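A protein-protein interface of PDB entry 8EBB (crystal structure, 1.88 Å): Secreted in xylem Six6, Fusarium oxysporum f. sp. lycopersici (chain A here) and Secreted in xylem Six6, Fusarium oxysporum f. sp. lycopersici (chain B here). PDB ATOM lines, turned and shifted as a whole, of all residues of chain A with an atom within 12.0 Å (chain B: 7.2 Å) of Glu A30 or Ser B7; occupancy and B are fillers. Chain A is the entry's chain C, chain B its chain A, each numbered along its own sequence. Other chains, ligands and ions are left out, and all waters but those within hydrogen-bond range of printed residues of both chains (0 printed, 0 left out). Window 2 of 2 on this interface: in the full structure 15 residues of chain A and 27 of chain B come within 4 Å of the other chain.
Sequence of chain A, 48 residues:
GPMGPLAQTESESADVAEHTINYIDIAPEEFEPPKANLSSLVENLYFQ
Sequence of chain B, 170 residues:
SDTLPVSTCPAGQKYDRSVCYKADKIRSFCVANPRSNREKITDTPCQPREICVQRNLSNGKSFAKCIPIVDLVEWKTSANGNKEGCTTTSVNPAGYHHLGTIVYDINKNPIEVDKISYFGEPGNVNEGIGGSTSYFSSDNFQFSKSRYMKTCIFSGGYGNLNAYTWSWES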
ATOM      1  N   ASP A  25     -17.207  -4.312 -23.762  1.00  0.00           N
ATOM      2  CA  ASP A  25     -15.964  -4.804 -23.180  1.00  0.00           C
ATOM      3  C   ASP A  25     -15.793  -4.320 -21.752  1.00  0.00           C
ATOM      4  O   ASP A  25     -16.042  -3.153 -21.443  1.00  0.00           O
ATOM      5  CB  ASP A  25     -14.758  -4.338 -23.996  1.00  0.00           C
ATOM      6  CG  ASP A  25     -13.525  -5.164 -23.709  1.00  0.00           C
ATOM      7  OD1 ASP A  25     -13.571  -6.371 -24.024  1.00  0.00           O
ATOM      8  OD2 ASP A  25     -12.532  -4.634 -23.140  1.00  0.00           O
ATOM      9  N   ILE A  26     -15.351  -5.220 -20.874  1.00  0.00           N
ATOM     10  CA  ILE A  26     -14.991  -4.861 -19.507  1.00  0.00           C
ATOM     11  C   ILE A  26     -13.644  -5.507 -19.202  1.00  0.00           C
ATOM     12  O   ILE A  26     -13.469  -6.710 -19.435  1.00  0.00           O
ATOM     13  CB  ILE A  26     -16.058  -5.300 -18.481  1.00  0.00           C
ATOM     14  CG1 ILE A  26     -17.396  -4.590 -18.749  1.00  0.00           C
ATOM     15  CG2 ILE A  26     -15.586  -5.020 -17.060  1.00  0.00           C
ATOM     16  CD1 ILE A  26     -18.518  -5.040 -17.883  1.00  0.00           C
ATOM     17  N   ALA A  27     -12.692  -4.708 -18.717  1.00  0.00           N
ATOM     18  CA  ALA A  27     -11.358  -5.236 -18.414  1.00  0.00           C
ATOM     19  C   ALA A  27     -11.422  -6.156 -17.200  1.00  0.00           C
ATOM     20  O   ALA A  27     -12.141  -5.864 -16.238  1.00  0.00           O
ATOM     21  CB  ALA A  27     -10.368  -4.101 -18.146  1.00  0.00           C
ATOM     22  N   PRO A  28     -10.696  -7.278 -17.211  1.00  0.00           N
ATOM     23  CA  PRO A  28     -10.721  -8.162 -16.043  1.00  0.00           C
ATOM     24  C   PRO A  28     -10.242  -7.427 -14.803  1.00  0.00           C
ATOM     25  O   PRO A  28      -9.437  -6.487 -14.872  1.00  0.00           O
ATOM     26  CB  PRO A  28      -9.771  -9.308 -16.426  1.00  0.00           C
ATOM     27  CG  PRO A  28      -9.727  -9.293 -17.919  1.00  0.00           C
ATOM     28  CD  PRO A  28      -9.938  -7.849 -18.339  1.00  0.00           C
ATOM     29  N   GLU A  29     -10.760  -7.870 -13.660  1.00  0.00           N
ATOM     30  CA  GLU A  29     -10.329  -7.341 -12.376  1.00  0.00           C
ATOM     31  C   GLU A  29      -8.813  -7.336 -12.226  1.00  0.00           C
ATOM     32  O   GLU A  29      -8.250  -6.426 -11.605  1.00  0.00           O
ATOM     33  CB  GLU A  29     -10.954  -8.142 -11.244  1.00  0.00           C
ATOM     34  CG  GLU A  29     -11.169  -7.290 -10.042  1.00  0.00           C
ATOM     35  CD  GLU A  29     -11.774  -8.028  -8.897  1.00  0.00           C
ATOM     36  OE1 GLU A  29     -11.341  -9.158  -8.576  1.00  0.00           O
ATOM     37  OE2 GLU A  29     -12.666  -7.433  -8.271  1.00  0.00           O
ATOM     38  N   GLU A  30      -8.136  -8.350 -12.763  1.00  0.00           N
ATOM     39  CA  GLU A  30      -6.703  -8.441 -12.521  1.00  0.00           C
ATOM     40  C   GLU A  30      -5.936  -7.290 -13.169  1.00  0.00           C
ATOM     41  O   GLU A  30      -4.780  -7.056 -12.806  1.00  0.00           O
ATOM     42  CB  GLU A  30      -6.174  -9.792 -13.009  1.00  0.00           C
ATOM     43  CG  GLU A  30      -5.599  -9.802 -14.418  1.00  0.00           C
ATOM     44  CD  GLU A  30      -5.736 -11.156 -15.113  1.00  0.00           C
ATOM     45  OE1 GLU A  30      -4.690 -11.713 -15.548  1.00  0.00           O
ATOM     46  OE2 GLU A  30      -6.894 -11.619 -15.286  1.00  0.00           O
ATOM     47  N   PHE A  31      -6.553  -6.561 -14.102  1.00  0.00           N
ATOM     48  CA  PHE A  31      -5.952  -5.380 -14.715  1.00  0.00           C
ATOM     49  C   PHE A  31      -6.543  -4.072 -14.204  1.00  0.00           C
ATOM     50  O   PHE A  31      -5.830  -3.065 -14.139  1.00  0.00           O
ATOM     51  CB  PHE A  31      -6.116  -5.421 -16.241  1.00  0.00           C
ATOM     52  CG  PHE A  31      -5.482  -6.611 -16.889  1.00  0.00           C
ATOM     53  CD1 PHE A  31      -4.136  -6.617 -17.172  1.00  0.00           C
ATOM     54  CD2 PHE A  31      -6.239  -7.723 -17.229  1.00  0.00           C
ATOM     55  CE1 PHE A  31      -3.540  -7.721 -17.768  1.00  0.00           C
ATOM     56  CE2 PHE A  31      -5.652  -8.822 -17.839  1.00  0.00           C
ATOM     57  CZ  PHE A  31      -4.301  -8.824 -18.104  1.00  0.00           C
ATOM     58  N   GLU A  32      -7.834  -4.067 -13.853  1.00  0.00           N
ATOM     59  CA  GLU A  32      -8.555  -2.892 -13.360  1.00  0.00           C
ATOM     60  C   GLU A  32      -9.143  -3.259 -12.002  1.00  0.00           C
ATOM     61  O   GLU A  32     -10.320  -3.639 -11.910  1.00  0.00           O
ATOM     62  CB  GLU A  32      -9.656  -2.454 -14.326  1.00  0.00           C
ATOM     63  CG  GLU A  32     -10.137  -1.001 -14.148  1.00  0.00           C
ATOM     64  CD  GLU A  32     -11.129  -0.557 -15.219  1.00  0.00           C
ATOM     65  OE1 GLU A  32     -11.963  -1.390 -15.656  1.00  0.00           O
ATOM     66  OE2 GLU A  32     -11.078   0.632 -15.623  1.00  0.00           O
ATOM     67  N   PRO A  33      -8.347  -3.175 -10.924  1.00  0.00           N
ATOM     68  CA  PRO A  33      -8.816  -3.544  -9.578  1.00  0.00           C
ATOM     69  C   PRO A  33      -9.843  -2.559  -8.998  1.00  0.00           C
ATOM     70  O   PRO A  33     -10.639  -2.929  -8.123  1.00  0.00           O
ATOM     71  CB  PRO A  33      -7.531  -3.557  -8.738  1.00  0.00           C
ATOM     72  CG  PRO A  33      -6.410  -3.086  -9.636  1.00  0.00           C
ATOM     73  CD  PRO A  33      -6.976  -2.633 -10.938  1.00  0.00           C
ATOM     74  N   LEU B   4      -6.358 -11.559 -24.463  1.00  0.00           N
ATOM     75  CA  LEU B   4      -5.984 -10.640 -23.408  1.00  0.00           C
ATOM     76  C   LEU B   4      -4.486 -10.408 -23.412  1.00  0.00           C
ATOM     77  O   LEU B   4      -3.716 -11.237 -23.910  1.00  0.00           O
ATOM     78  CB  LEU B   4      -6.419 -11.203 -22.056  1.00  0.00           C
ATOM     79  CG  LEU B   4      -7.930 -11.078 -21.839  1.00  0.00           C
ATOM     80  CD1 LEU B   4      -8.383 -11.756 -20.563  1.00  0.00           C
ATOM     81  CD2 LEU B   4      -8.300  -9.598 -21.826  1.00  0.00           C
ATOM     82  N   PRO B   5      -4.028  -9.282 -22.870  1.00  0.00           N
ATOM     83  CA  PRO B   5      -2.590  -9.109 -22.662  1.00  0.00           C
ATOM     84  C   PRO B   5      -2.113 -10.080 -21.595  1.00  0.00           C
ATOM     85  O   PRO B   5      -2.885 -10.566 -20.772  1.00  0.00           O
ATOM     86  CB  PRO B   5      -2.460  -7.656 -22.195  1.00  0.00           C
ATOM     87  CG  PRO B   5      -3.792  -7.352 -21.569  1.00  0.00           C
ATOM     88  CD  PRO B   5      -4.813  -8.165 -22.311  1.00  0.00           C
ATOM     89  N   VAL B   6      -0.824 -10.361 -21.620  1.00  0.00           N
ATOM     90  CA  VAL B   6      -0.220 -11.279 -20.665  1.00  0.00           C
ATOM     91  C   VAL B   6       0.136 -10.501 -19.402  1.00  0.00           C
ATOM     92  O   VAL B   6       0.849  -9.497 -19.460  1.00  0.00           O
ATOM     93  CB  VAL B   6       1.013 -11.963 -21.270  1.00  0.00           C
ATOM     94  CG1 VAL B   6       1.897 -12.555 -20.158  1.00  0.00           C
ATOM     95  CG2 VAL B   6       0.569 -13.046 -22.278  1.00  0.00           C
ATOM     96  N   SER B   7      -0.377 -10.953 -18.260  1.00  0.00           N
ATOM     97  CA  SER B   7      -0.167 -10.271 -16.988  1.00  0.00           C
ATOM     98  C   SER B   7       0.954 -10.877 -16.141  1.00  0.00           C
ATOM     99  O   SER B   7       1.281 -10.319 -15.086  1.00  0.00           O
ATOM    100  CB  SER B   7      -1.478 -10.256 -16.182  1.00  0.00           C
ATOM    101  OG  SER B   7      -1.833 -11.545 -15.687  1.00  0.00           O
ATOM    102  N   THR B   8       1.550 -11.988 -16.566  1.00  0.00           N
ATOM    103  CA  THR B   8       2.584 -12.656 -15.782  1.00  0.00           C
ATOM    104  C   THR B   8       3.951 -12.041 -16.067  1.00  0.00           C
ATOM    105  O   THR B   8       4.252 -11.650 -17.201  1.00  0.00           O
ATOM    106  CB  THR B   8       2.602 -14.157 -16.077  1.00  0.00           C
ATOM    107  OG1 THR B   8       2.781 -14.369 -17.482  1.00  0.00           O
ATOM    108  CG2 THR B   8       1.304 -14.803 -15.631  1.00  0.00           C
ATOM    109  N   CYS B   9       4.774 -11.948 -15.029  1.00  0.00           N
ATOM    110  CA  CYS B   9       6.065 -11.288 -15.111  1.00  0.00           C
ATOM    111  C   CYS B   9       7.111 -12.129 -14.399  1.00  0.00           C
ATOM    112  O   CYS B   9       6.774 -12.961 -13.551  1.00  0.00           O
ATOM    113  CB  CYS B   9       6.010  -9.886 -14.494  1.00  0.00           C
ATOM    114  SG  CYS B   9       5.010  -8.720 -15.461  1.00  0.00           S
ATOM    115  N   GLN B  13       9.301  -8.577 -10.833  1.00  0.00           N
ATOM    116  CA  GLN B  13       8.700  -7.644 -11.771  1.00  0.00           C
ATOM    117  C   GLN B  13       7.189  -7.731 -11.639  1.00  0.00           C
ATOM    118  O   GLN B  13       6.659  -8.769 -11.228  1.00  0.00           O
ATOM    119  CB  GLN B  13       9.139  -7.952 -13.211  1.00  0.00           C
ATOM    120  CG  GLN B  13      10.651  -8.060 -13.371  1.00  0.00           C
ATOM    121  CD  GLN B  13      11.080  -8.207 -14.813  1.00  0.00           C
ATOM    122  OE1 GLN B  13      10.279  -8.042 -15.734  1.00  0.00           O
ATOM    123  NE2 GLN B  13      12.351  -8.543 -15.022  1.00  0.00           N
ATOM    124  N   LYS B  14       6.500  -6.631 -11.978  1.00  0.00           N
ATOM    125  CA  LYS B  14       5.040  -6.547 -11.905  1.00  0.00           C
ATOM    126  C   LYS B  14       4.504  -6.005 -13.217  1.00  0.00           C
ATOM    127  O   LYS B  14       5.128  -5.123 -13.826  1.00  0.00           O
ATOM    128  CB  LYS B  14       4.550  -5.626 -10.769  1.00  0.00           C
ATOM    129  CG  LYS B  14       4.421  -6.299  -9.415  1.00  0.00           C
ATOM    130  CD  LYS B  14       5.183  -5.561  -8.329  1.00  0.00           C
ATOM    131  CE  LYS B  14       5.632  -6.513  -7.211  1.00  0.00           C
ATOM    132  NZ  LYS B  14       6.981  -6.144  -6.690  1.00  0.00           N
ATOM    133  N   TYR B  15       3.334  -6.510 -13.627  1.00  0.00           N
ATOM    134  CA  TYR B  15       2.689  -6.015 -14.839  1.00  0.00           C
ATOM    135  C   TYR B  15       2.355  -4.543 -14.666  1.00  0.00           C
ATOM    136  O   TYR B  15       1.792  -4.140 -13.647  1.00  0.00           O
ATOM    137  CB  TYR B  15       1.415  -6.814 -15.144  1.00  0.00           C
ATOM    138  CG  TYR B  15       0.528  -6.168 -16.201  1.00  0.00           C
ATOM    139  CD1 TYR B  15      -0.474  -5.264 -15.844  1.00  0.00           C
ATOM    140  CD2 TYR B  15       0.696  -6.456 -17.548  1.00  0.00           C
ATOM    141  CE1 TYR B  15      -1.290  -4.663 -16.806  1.00  0.00           C
ATOM    142  CE2 TYR B  15      -0.112  -5.854 -18.524  1.00  0.00           C
ATOM    143  CZ  TYR B  15      -1.100  -4.961 -18.140  1.00  0.00           C
ATOM    144  OH  TYR B  15      -1.918  -4.367 -19.075  1.00  0.00           O
ATOM    145  N   ASP B  16       2.690  -3.736 -15.666  1.00  0.00           N
ATOM    146  CA  ASP B  16       2.444  -2.303 -15.589  1.00  0.00           C
ATOM    147  C   ASP B  16       1.362  -1.814 -16.541  1.00  0.00           C
ATOM    148  O   ASP B  16       0.478  -1.067 -16.120  1.00  0.00           O
ATOM    149  CB  ASP B  16       3.742  -1.529 -15.862  1.00  0.00           C
ATOM    150  CG  ASP B  16       3.578  -0.038 -15.653  1.00  0.00           C
ATOM    151  OD1 ASP B  16       3.268   0.354 -14.521  1.00  0.00           O
ATOM    152  OD2 ASP B  16       3.738   0.740 -16.619  1.00  0.00           O
ATOM    153  N   SER B  28       2.656  -6.195 -23.773  1.00  0.00           N
ATOM    154  CA  SER B  28       2.559  -5.977 -22.335  1.00  0.00           C
ATOM    155  C   SER B  28       3.934  -5.636 -21.771  1.00  0.00           C
ATOM    156  O   SER B  28       4.957  -6.136 -22.254  1.00  0.00           O
ATOM    157  CB  SER B  28       2.021  -7.217 -21.608  1.00  0.00           C
ATOM    158  OG  SER B  28       0.798  -7.673 -22.160  1.00  0.00           O
ATOM    159  N   CYS B  30       6.211  -5.387 -18.193  1.00  0.00           N
ATOM    160  CA  CYS B  30       6.547  -5.564 -16.792  1.00  0.00           C
ATOM    161  C   CYS B  30       7.529  -4.481 -16.348  1.00  0.00           C
ATOM    162  O   CYS B  30       8.252  -3.899 -17.155  1.00  0.00           O
ATOM    163  CB  CYS B  30       7.170  -6.935 -16.578  1.00  0.00           C
ATOM    164  SG  CYS B  30       6.118  -8.280 -17.113  1.00  0.00           S
ATOM    165  N   THR B  42       6.247  -8.481 -23.496  1.00  0.00           N
ATOM    166  CA  THR B  42       5.669  -9.676 -24.096  1.00  0.00           C
ATOM    167  C   THR B  42       4.697  -9.278 -25.195  1.00  0.00           C
ATOM    168  O   THR B  42       3.768  -8.509 -24.948  1.00  0.00           O
ATOM    169  CB  THR B  42       4.951 -10.519 -23.049  1.00  0.00           C
ATOM    170  OG1 THR B  42       5.853 -10.831 -21.975  1.00  0.00           O
ATOM    171  CG2 THR B  42       4.420 -11.807 -23.680  1.00  0.00           C
ATOM    172  N   LEU B  57      -7.154   2.818 -18.317  1.00  0.00           N
ATOM    173  CA  LEU B  57      -7.931   2.321 -17.195  1.00  0.00           C
ATOM    174  C   LEU B  57      -8.127   3.426 -16.166  1.00  0.00           C
ATOM    175  O   LEU B  57      -7.446   4.460 -16.198  1.00  0.00           O
ATOM    176  CB  LEU B  57      -7.223   1.138 -16.547  1.00  0.00           C
ATOM    177  CG  LEU B  57      -7.116  -0.087 -17.439  1.00  0.00           C
ATOM    178  CD1 LEU B  57      -6.427  -1.246 -16.687  1.00  0.00           C
ATOM    179  CD2 LEU B  57      -8.483  -0.477 -17.944  1.00  0.00           C
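OE1 of Glu A30 sits at hydrogen-bond distance from OG of Ser B7 (2.9 Å).
N of Tyr B15 lies within hydrogen-bond range of SG of Cys B9 (3.3 Å).
SG of Cys B9 is disulfide-bonded to SG of Cys B30 (2.0 Å).
Leu B4 touches Pro A28.
CZ of Phe A31 touches O of Pro B5 (3.5 Å).
CB of Ser B7 touches CE1 of Phe A31, 3.6 Å away.
CD1 of Phe A31 touches CE1 of Tyr B15, 3.5 Å away.
Leu B57 touches Phe A31 (CD1 to O, 3.2 Å).
Glu A32 touches Leu B57.
Glu A30 touches just one residue of chain B: Ser B7 (2.9 Å).
Pro B5 touches one residue of chain A.
Val B6 touches none of the printed residues of chain A.
Cys B9 touches none of the printed residues of chain A.
Of the printed residues of chain A, Tyr B15 touches Phe A31.
Of the printed residues of chain A, Leu B57 touches Phe A31 and Glu A32.
Printed residues of chain B within 4 Å of Glu A32: Leu B57 (3.7 Å).
Printed residues of chain B within 4 Å of Pro A28: Leu B4.
Of the printed residues of chain A, Leu B4 touches Pro A28 (3.9 Å).
Cys B30 touches none of the printed residues of chain A.
Asp A25 touches none of the printed residues of chain B.
The nearest residue of chain B that does not touch Glu A30 is Leu B4 (5.5 Å).
The nearest residue of chain A that does not touch Ser B7 is Pro A28 (8.3 Å).
Printed residues of chain B that touch a printed residue of chain A: Leu B4, Pro B5, Ser B7, Tyr B15 and Leu B57.
Hydrophobic or aromatic side chains of chain B that line the printed part of chain A: Leu B4, Pro B5, Tyr B15 and Leu B57.
Hydrophobic or aromatic side chains of chain A within 4 Å of the printed part of chain B: Pro A28 and Phe A31.
Among the printed residues, 7 pairs touch across the chains.
Among the printed residues, no Asp or Glu carboxylate lies within 4 Å of a Lys or Arg side-chain nitrogen of the other chain.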
